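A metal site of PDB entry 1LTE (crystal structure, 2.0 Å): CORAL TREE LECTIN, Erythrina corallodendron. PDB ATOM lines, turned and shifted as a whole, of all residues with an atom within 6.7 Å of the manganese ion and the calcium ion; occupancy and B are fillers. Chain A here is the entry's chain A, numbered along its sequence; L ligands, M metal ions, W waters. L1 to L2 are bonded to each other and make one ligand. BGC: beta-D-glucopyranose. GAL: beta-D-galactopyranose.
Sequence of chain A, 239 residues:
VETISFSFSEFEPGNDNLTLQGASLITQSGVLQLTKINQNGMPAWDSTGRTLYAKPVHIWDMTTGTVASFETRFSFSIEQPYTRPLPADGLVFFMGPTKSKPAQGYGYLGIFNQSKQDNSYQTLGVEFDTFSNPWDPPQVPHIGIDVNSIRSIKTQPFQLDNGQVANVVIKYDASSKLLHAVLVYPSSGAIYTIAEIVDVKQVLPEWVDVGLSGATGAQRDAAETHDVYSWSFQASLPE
Water W1 is bound to the calcium ion (2.3 Å).
Water W4 is bound to the calcium ion.
The calcium ion is bound by OD2 of Asp 136 (2.4 Å).
OD1 of Asn 133 binds the calcium ion (2.4 Å).
The calcium ion is bound by the side-chain carboxylate (OD1) of Asp 129, 2.5 Å away.
The side-chain carboxylate (OD2) of Asp 129 is bound to the calcium ion (2.5 Å).
The calcium ion is bound by O of Phe 131 (2.5 Å).
The calcium ion has seven donor atoms within binding distance.
The backbone NH (N) of Glu 127 sits at hydrogen-bond distance from the backbone carbonyl oxygen (O) of Gly 144 (2.9 Å).
Water W2 bridges the side-chain carboxylate of Glu 127 (2.7 Å) and the backbone carbonyl oxygen of Ile 150 (2.8 Å).
Water W4 bridges the backbone carbonyl oxygen (O) of Gly 107 (2.8 Å) and the indole nitrogen (NE1) of Trp 135 (3.1 Å).
The manganese ion is bound by water W3 (2.1 Å), water W2 (2.2 Å), the side-chain carboxylate (OD1) of Asp 136 (2.2 Å), the side-chain carboxylate (OE2) of Glu 127 (2.2 Å), the side-chain carboxylate (OD2) of Asp 129 (2.2 Å) and a ring nitrogen (NE2) of His 142 (2.4 Å).
The side-chain amide nitrogen (ND2) of Asn 133 is in hydrogen-bond range of an oxygen (O3) of GAL L2, 3.0 Å away.
An oxygen (O3) of GAL L2 sits at hydrogen-bond distance from the backbone NH (N) of Gly 107 (2.9 Å).
An oxygen (O3) of GAL L2 lies within hydrogen-bond range of the side-chain carboxylate (OD1) of Asp 89, at 2.8 Å.
Within 4 Å of the manganese ion: Glu 127, Asp 129, Asp 136 and His 142.
Of the 23 residues printed, 4 come within 4 Å of the calcium ion.
The nearest printed residue that does not touch the calcium ion is Trp 135 (4.4 Å).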
ATOM      1  N   ASP A  89      11.130   0.285 -20.568  1.00  0.00           N
ATOM      2  CA  ASP A  89      10.247  -0.848 -20.246  1.00  0.00           C
ATOM      3  C   ASP A  89       9.157  -0.482 -19.264  1.00  0.00           C
ATOM      4  O   ASP A  89       8.093  -1.104 -19.283  1.00  0.00           O
ATOM      5  CB  ASP A  89      11.040  -2.035 -19.679  1.00  0.00           C
ATOM      6  CG  ASP A  89      11.520  -2.953 -20.799  1.00  0.00           C
ATOM      7  OD1 ASP A  89      10.761  -3.766 -21.347  1.00  0.00           O
ATOM      8  OD2 ASP A  89      12.679  -2.868 -21.157  1.00  0.00           O
ATOM      9  N   TYR A 106      15.162  -4.482 -17.826  1.00  0.00           N
ATOM     10  CA  TYR A 106      14.325  -4.590 -19.025  1.00  0.00           C
ATOM     11  C   TYR A 106      12.912  -4.927 -18.597  1.00  0.00           C
ATOM     12  O   TYR A 106      12.463  -4.342 -17.605  1.00  0.00           O
ATOM     13  CB  TYR A 106      14.872  -5.674 -20.008  1.00  0.00           C
ATOM     14  CG  TYR A 106      16.358  -5.605 -20.276  1.00  0.00           C
ATOM     15  CD1 TYR A 106      16.959  -4.414 -20.619  1.00  0.00           C
ATOM     16  CD2 TYR A 106      17.103  -6.740 -20.113  1.00  0.00           C
ATOM     17  CE1 TYR A 106      18.323  -4.355 -20.812  1.00  0.00           C
ATOM     18  CE2 TYR A 106      18.450  -6.699 -20.302  1.00  0.00           C
ATOM     19  CZ  TYR A 106      19.053  -5.513 -20.658  1.00  0.00           C
ATOM     20  OH  TYR A 106      20.409  -5.515 -20.841  1.00  0.00           O
ATOM     21  N   GLY A 107      12.207  -5.863 -19.260  1.00  0.00           N
ATOM     22  CA  GLY A 107      10.850  -6.247 -18.895  1.00  0.00           C
ATOM     23  C   GLY A 107      10.695  -6.780 -17.485  1.00  0.00           C
ATOM     24  O   GLY A 107       9.582  -6.875 -16.994  1.00  0.00           O
ATOM     25  N   TYR A 108      11.757  -7.136 -16.772  1.00  0.00           N
ATOM     26  CA  TYR A 108      11.595  -7.630 -15.405  1.00  0.00           C
ATOM     27  C   TYR A 108      11.543  -6.487 -14.416  1.00  0.00           C
ATOM     28  O   TYR A 108      11.357  -6.697 -13.199  1.00  0.00           O
ATOM     29  CB  TYR A 108      12.713  -8.574 -15.053  1.00  0.00           C
ATOM     30  CG  TYR A 108      12.667  -9.787 -15.967  1.00  0.00           C
ATOM     31  CD1 TYR A 108      11.536 -10.574 -16.044  1.00  0.00           C
ATOM     32  CD2 TYR A 108      13.760 -10.062 -16.753  1.00  0.00           C
ATOM     33  CE1 TYR A 108      11.495 -11.629 -16.918  1.00  0.00           C
ATOM     34  CE2 TYR A 108      13.705 -11.116 -17.631  1.00  0.00           C
ATOM     35  CZ  TYR A 108      12.581 -11.891 -17.703  1.00  0.00           C
ATOM     36  OH  TYR A 108      12.541 -12.936 -18.605  1.00  0.00           O
ATOM     37  N   LEU A 109      11.780  -5.276 -14.938  1.00  0.00           N
ATOM     38  CA  LEU A 109      11.722  -4.006 -14.230  1.00  0.00           C
ATOM     39  C   LEU A 109      12.578  -3.804 -12.982  1.00  0.00           C
ATOM     40  O   LEU A 109      12.247  -2.974 -12.139  1.00  0.00           O
ATOM     41  CB  LEU A 109      10.219  -3.745 -13.917  1.00  0.00           C
ATOM     42  CG  LEU A 109       9.165  -3.793 -15.047  1.00  0.00           C
ATOM     43  CD1 LEU A 109       7.773  -3.639 -14.458  1.00  0.00           C
ATOM     44  CD2 LEU A 109       9.407  -2.688 -16.065  1.00  0.00           C
ATOM     45  N   GLU A 127       2.791  -2.220 -11.420  1.00  0.00           N
ATOM     46  CA  GLU A 127       3.555  -1.717 -12.555  1.00  0.00           C
ATOM     47  C   GLU A 127       2.803  -0.807 -13.510  1.00  0.00           C
ATOM     48  O   GLU A 127       1.561  -0.757 -13.530  1.00  0.00           O
ATOM     49  CB  GLU A 127       4.109  -2.898 -13.343  1.00  0.00           C
ATOM     50  CG  GLU A 127       2.981  -3.761 -13.898  1.00  0.00           C
ATOM     51  CD  GLU A 127       3.413  -4.823 -14.884  1.00  0.00           C
ATOM     52  OE1 GLU A 127       4.404  -5.506 -14.653  1.00  0.00           O
ATOM     53  OE2 GLU A 127       2.764  -4.951 -15.933  1.00  0.00           O
ATOM     54  N   ASP A 129       3.644  -0.545 -17.119  1.00  0.00           N
ATOM     55  CA  ASP A 129       4.382  -1.228 -18.158  1.00  0.00           C
ATOM     56  C   ASP A 129       4.208  -0.647 -19.554  1.00  0.00           C
ATOM     57  O   ASP A 129       3.091  -0.572 -20.066  1.00  0.00           O
ATOM     58  CB  ASP A 129       3.920  -2.694 -18.096  1.00  0.00           C
ATOM     59  CG  ASP A 129       4.805  -3.670 -18.868  1.00  0.00           C
ATOM     60  OD1 ASP A 129       5.555  -3.271 -19.754  1.00  0.00           O
ATOM     61  OD2 ASP A 129       4.738  -4.844 -18.573  1.00  0.00           O
ATOM     62  N   THR A 130       5.309  -0.279 -20.188  1.00  0.00           N
ATOM     63  CA  THR A 130       5.228   0.351 -21.500  1.00  0.00           C
ATOM     64  C   THR A 130       5.649  -0.530 -22.665  1.00  0.00           C
ATOM     65  O   THR A 130       5.540  -0.054 -23.804  1.00  0.00           O
ATOM     66  CB  THR A 130       6.079   1.638 -21.519  1.00  0.00           C
ATOM     67  OG1 THR A 130       7.422   1.243 -21.274  1.00  0.00           O
ATOM     68  CG2 THR A 130       5.629   2.648 -20.482  1.00  0.00           C
ATOM     69  N   PHE A 131       6.079  -1.780 -22.453  1.00  0.00           N
ATOM     70  CA  PHE A 131       6.500  -2.609 -23.570  1.00  0.00           C
ATOM     71  C   PHE A 131       5.839  -3.973 -23.461  1.00  0.00           C
ATOM     72  O   PHE A 131       5.931  -4.586 -22.422  1.00  0.00           O
ATOM     73  CB  PHE A 131       8.012  -2.745 -23.550  1.00  0.00           C
ATOM     74  CG  PHE A 131       8.516  -3.635 -24.669  1.00  0.00           C
ATOM     75  CD1 PHE A 131       8.727  -3.092 -25.921  1.00  0.00           C
ATOM     76  CD2 PHE A 131       8.733  -4.991 -24.469  1.00  0.00           C
ATOM     77  CE1 PHE A 131       9.125  -3.898 -26.967  1.00  0.00           C
ATOM     78  CE2 PHE A 131       9.133  -5.787 -25.518  1.00  0.00           C
ATOM     79  CZ  PHE A 131       9.331  -5.244 -26.774  1.00  0.00           C
ATOM     80  N   SER A 132       5.193  -4.504 -24.501  1.00  0.00           N
ATOM     81  CA  SER A 132       4.566  -5.794 -24.411  1.00  0.00           C
ATOM     82  C   SER A 132       5.514  -6.975 -24.635  1.00  0.00           C
ATOM     83  O   SER A 132       6.014  -7.241 -25.738  1.00  0.00           O
ATOM     84  CB  SER A 132       3.434  -5.810 -25.421  1.00  0.00           C
ATOM     85  OG  SER A 132       2.585  -6.929 -25.288  1.00  0.00           O
ATOM     86  N   ASN A 133       5.857  -7.647 -23.541  1.00  0.00           N
ATOM     87  CA  ASN A 133       6.725  -8.813 -23.528  1.00  0.00           C
ATOM     88  C   ASN A 133       5.903 -10.080 -23.821  1.00  0.00           C
ATOM     89  O   ASN A 133       4.682  -9.981 -23.819  1.00  0.00           O
ATOM     90  CB  ASN A 133       7.365  -8.974 -22.169  1.00  0.00           C
ATOM     91  CG  ASN A 133       8.398  -7.919 -21.863  1.00  0.00           C
ATOM     92  OD1 ASN A 133       8.130  -6.891 -21.254  1.00  0.00           O
ATOM     93  ND2 ASN A 133       9.617  -8.084 -22.293  1.00  0.00           N
ATOM     94  N   TRP A 135       4.881 -12.373 -21.977  1.00  0.00           N
ATOM     95  CA  TRP A 135       3.970 -12.599 -20.879  1.00  0.00           C
ATOM     96  C   TRP A 135       2.958 -11.486 -20.716  1.00  0.00           C
ATOM     97  O   TRP A 135       2.052 -11.619 -19.896  1.00  0.00           O
ATOM     98  CB  TRP A 135       4.763 -12.743 -19.567  1.00  0.00           C
ATOM     99  CG  TRP A 135       5.701 -11.578 -19.251  1.00  0.00           C
ATOM    100  CD1 TRP A 135       5.261 -10.403 -18.689  1.00  0.00           C
ATOM    101  CD2 TRP A 135       7.047 -11.564 -19.507  1.00  0.00           C
ATOM    102  NE1 TRP A 135       6.328  -9.656 -18.608  1.00  0.00           N
ATOM    103  CE2 TRP A 135       7.412 -10.309 -19.059  1.00  0.00           C
ATOM    104  CE3 TRP A 135       7.977 -12.439 -20.039  1.00  0.00           C
ATOM    105  CZ2 TRP A 135       8.719  -9.890 -19.151  1.00  0.00           C
ATOM    106  CZ3 TRP A 135       9.289 -12.018 -20.123  1.00  0.00           C
ATOM    107  CH2 TRP A 135       9.655 -10.753 -19.679  1.00  0.00           C
ATOM    108  N   ASP A 136       3.036 -10.403 -21.466  1.00  0.00           N
ATOM    109  CA  ASP A 136       2.108  -9.303 -21.296  1.00  0.00           C
ATOM    110  C   ASP A 136       0.878  -9.412 -22.150  1.00  0.00           C
ATOM    111  O   ASP A 136       0.927 -10.052 -23.201  1.00  0.00           O
ATOM    112  CB  ASP A 136       2.789  -8.001 -21.625  1.00  0.00           C
ATOM    113  CG  ASP A 136       3.716  -7.523 -20.527  1.00  0.00           C
ATOM    114  OD1 ASP A 136       3.359  -7.602 -19.365  1.00  0.00           O
ATOM    115  OD2 ASP A 136       4.818  -7.119 -20.860  1.00  0.00           O
ATOM    116  N   PRO A 137      -0.237  -8.768 -21.812  1.00  0.00           N
ATOM    117  CA  PRO A 137      -1.311  -8.499 -22.742  1.00  0.00           C
ATOM    118  C   PRO A 137      -0.787  -7.662 -23.904  1.00  0.00           C
ATOM    119  O   PRO A 137       0.189  -6.936 -23.729  1.00  0.00           O
ATOM    120  CB  PRO A 137      -2.344  -7.791 -21.918  1.00  0.00           C
ATOM    121  CG  PRO A 137      -1.517  -7.081 -20.890  1.00  0.00           C
ATOM    122  CD  PRO A 137      -0.504  -8.160 -20.516  1.00  0.00           C
ATOM    123  N   VAL A 140      -0.306  -1.855 -24.520  1.00  0.00           N
ATOM    124  CA  VAL A 140       0.632  -1.140 -23.669  1.00  0.00           C
ATOM    125  C   VAL A 140       0.393   0.345 -23.940  1.00  0.00           C
ATOM    126  O   VAL A 140      -0.020   0.667 -25.064  1.00  0.00           O
ATOM    127  CB  VAL A 140       2.136  -1.465 -23.952  1.00  0.00           C
ATOM    128  CG1 VAL A 140       2.410  -2.814 -23.332  1.00  0.00           C
ATOM    129  CG2 VAL A 140       2.501  -1.442 -25.403  1.00  0.00           C
ATOM    130  N   HIS A 142       0.143  -0.369 -19.704  1.00  0.00           N
ATOM    131  CA  HIS A 142      -0.912  -0.935 -18.861  1.00  0.00           C
ATOM    132  C   HIS A 142      -0.415  -0.912 -17.418  1.00  0.00           C
ATOM    133  O   HIS A 142       0.786  -0.843 -17.128  1.00  0.00           O
ATOM    134  CB  HIS A 142      -1.293  -2.410 -19.237  1.00  0.00           C
ATOM    135  CG  HIS A 142      -0.167  -3.429 -19.355  1.00  0.00           C
ATOM    136  ND1 HIS A 142       0.462  -3.797 -20.456  1.00  0.00           N
ATOM    137  CD2 HIS A 142       0.375  -4.125 -18.303  1.00  0.00           C
ATOM    138  CE1 HIS A 142       1.376  -4.683 -20.142  1.00  0.00           C
ATOM    139  NE2 HIS A 142       1.307  -4.864 -18.850  1.00  0.00           N
ATOM    140  N   ILE A 143      -1.390  -0.790 -16.546  1.00  0.00           N
ATOM    141  CA  ILE A 143      -1.143  -0.835 -15.123  1.00  0.00           C
ATOM    142  C   ILE A 143      -1.270  -2.340 -14.832  1.00  0.00           C
ATOM    143  O   ILE A 143      -2.180  -2.982 -15.387  1.00  0.00           O
ATOM    144  CB  ILE A 143      -2.240  -0.104 -14.300  1.00  0.00           C
ATOM    145  CG1 ILE A 143      -2.468   1.310 -14.845  1.00  0.00           C
ATOM    146  CG2 ILE A 143      -1.791  -0.036 -12.823  1.00  0.00           C
ATOM    147  CD1 ILE A 143      -3.701   2.021 -14.270  1.00  0.00           C
ATOM    148  N   GLY A 144      -0.454  -2.947 -13.993  1.00  0.00           N
ATOM    149  CA  GLY A 144      -0.613  -4.373 -13.689  1.00  0.00           C
ATOM    150  C   GLY A 144      -0.358  -4.625 -12.203  1.00  0.00           C
ATOM    151  O   GLY A 144       0.355  -3.834 -11.567  1.00  0.00           O
ATOM    152  N   ASP A 146       1.255  -7.203  -9.761  1.00  0.00           N
ATOM    153  CA  ASP A 146       2.213  -8.306  -9.766  1.00  0.00           C
ATOM    154  C   ASP A 146       2.362  -8.929  -8.403  1.00  0.00           C
ATOM    155  O   ASP A 146       2.731  -8.248  -7.426  1.00  0.00           O
ATOM    156  CB  ASP A 146       3.568  -7.806 -10.224  1.00  0.00           C
ATOM    157  CG  ASP A 146       3.540  -7.115 -11.577  1.00  0.00           C
ATOM    158  OD1 ASP A 146       2.523  -7.177 -12.242  1.00  0.00           O
ATOM    159  OD2 ASP A 146       4.551  -6.517 -11.938  1.00  0.00           O
ATOM    160  N   ILE A 150       6.215 -11.353 -12.714  1.00  0.00           N
ATOM    161  CA  ILE A 150       6.091 -10.224 -13.637  1.00  0.00           C
ATOM    162  C   ILE A 150       4.802 -10.474 -14.487  1.00  0.00           C
ATOM    163  O   ILE A 150       4.301  -9.653 -15.216  1.00  0.00           O
ATOM    164  CB  ILE A 150       7.409 -10.167 -14.495  1.00  0.00           C
ATOM    165  CG1 ILE A 150       7.446  -8.850 -15.257  1.00  0.00           C
ATOM    166  CG2 ILE A 150       7.536 -11.339 -15.439  1.00  0.00           C
ATOM    167  CD1 ILE A 150       7.526  -7.588 -14.342  1.00  0.00           C
ATOM    168  N   ARG A 151       4.196 -11.651 -14.381  1.00  0.00           N
ATOM    169  CA  ARG A 151       2.991 -12.025 -15.118  1.00  0.00           C
ATOM    170  C   ARG A 151       1.853 -11.517 -14.241  1.00  0.00           C
ATOM    171  O   ARG A 151       1.429 -12.253 -13.349  1.00  0.00           O
ATOM    172  CB  ARG A 151       3.225 -13.517 -15.239  1.00  0.00           C
ATOM    173  CG  ARG A 151       2.292 -14.428 -15.977  1.00  0.00           C
ATOM    174  CD  ARG A 151       3.135 -15.534 -16.660  1.00  0.00           C
ATOM    175  NE  ARG A 151       4.072 -16.293 -15.837  1.00  0.00           N
ATOM    176  CZ  ARG A 151       3.790 -17.410 -15.161  1.00  0.00           C
ATOM    177  NH1 ARG A 151       2.562 -17.923 -15.098  1.00  0.00           N
ATOM    178  NH2 ARG A 151       4.763 -18.015 -14.480  1.00  0.00           N
ATOM    179  N   SER A 152       1.358 -10.287 -14.403  1.00  0.00           N
ATOM    180  CA  SER A 152       0.296  -9.714 -13.572  1.00  0.00           C
ATOM    181  C   SER A 152      -0.947 -10.536 -13.387  1.00  0.00           C
ATOM    182  O   SER A 152      -1.396 -11.222 -14.308  1.00  0.00           O
ATOM    183  CB  SER A 152      -0.163  -8.329 -14.112  1.00  0.00           C
ATOM    184  OG  SER A 152       1.039  -7.741 -14.539  1.00  0.00           O
ATOM    185  N   THR A 155      -4.620  -6.617 -15.134  1.00  0.00           N
ATOM    186  CA  THR A 155      -4.063  -5.593 -16.011  1.00  0.00           C
ATOM    187  C   THR A 155      -5.108  -4.539 -16.381  1.00  0.00           C
ATOM    188  O   THR A 155      -6.297  -4.875 -16.405  1.00  0.00           O
ATOM    189  CB  THR A 155      -3.521  -6.470 -17.160  1.00  0.00           C
ATOM    190  OG1 THR A 155      -2.112  -6.347 -17.041  1.00  0.00           O
ATOM    191  CG2 THR A 155      -4.082  -6.158 -18.515  1.00  0.00           C
HETATM  192  C2  BGC L   1      16.612  -7.948 -28.894  1.00  0.00           C
HETATM  193  C3  BGC L   1      16.175  -7.349 -27.566  1.00  0.00           C
HETATM  194  C4  BGC L   1      15.121  -8.335 -26.944  1.00  0.00           C
HETATM  195  C5  BGC L   1      15.659  -9.793 -26.836  1.00  0.00           C
HETATM  196  C6  BGC L   1      14.558 -10.867 -26.555  1.00  0.00           C
HETATM  197  C1  BGC L   1      17.220  -9.346 -28.689  1.00  0.00           C
HETATM  198  O1  BGC L   1      17.567  -9.918 -29.938  1.00  0.00           O
HETATM  199  O2  BGC L   1      17.512  -7.039 -29.514  1.00  0.00           O
HETATM  200  O3  BGC L   1      15.654  -6.046 -27.829  1.00  0.00           O
HETATM  201  O4  BGC L   1      14.811  -7.935 -25.586  1.00  0.00           O
HETATM  202  O5  BGC L   1      16.279 -10.213 -28.065  1.00  0.00           O
HETATM  203  O6  BGC L   1      13.253 -10.353 -26.411  1.00  0.00           O
HETATM  204  C1  GAL L   2      13.641  -7.145 -25.349  1.00  0.00           C
HETATM  205  C2  GAL L   2      13.396  -7.097 -23.826  1.00  0.00           C
HETATM  206  C3  GAL L   2      12.200  -6.191 -23.505  1.00  0.00           C
HETATM  207  C4  GAL L   2      12.517  -4.794 -24.072  1.00  0.00           C
HETATM  208  C5  GAL L   2      12.794  -4.866 -25.585  1.00  0.00           C
HETATM  209  C6  GAL L   2      13.205  -3.514 -26.190  1.00  0.00           C
HETATM  210  O2  GAL L   2      13.154  -8.362 -23.249  1.00  0.00           O
HETATM  211  O3  GAL L   2      11.965  -6.154 -22.086  1.00  0.00           O
HETATM  212  O4  GAL L   2      13.659  -4.272 -23.407  1.00  0.00           O
HETATM  213  O5  GAL L   2      13.848  -5.809 -25.848  1.00  0.00           O
HETATM  214  O6  GAL L   2      13.430  -3.710 -27.571  1.00  0.00           O
HETATM  215 MN    MN M   1       3.063  -6.106 -17.796  1.00  0.00          MN
HETATM  216 CA    CA M   2       6.457  -5.507 -20.190  1.00  0.00          CA
HETATM  217  O   HOH W   1       8.315  -4.136 -20.053  1.00  0.00           O
HETATM  218  O   HOH W   2       4.532  -7.277 -16.677  1.00  0.00           O
HETATM  219  O   HOH W   3       1.523  -7.464 -17.186  1.00  0.00           O
HETATM  220  O   HOH W   4       7.060  -6.633 -18.228  1.00  0.00           O
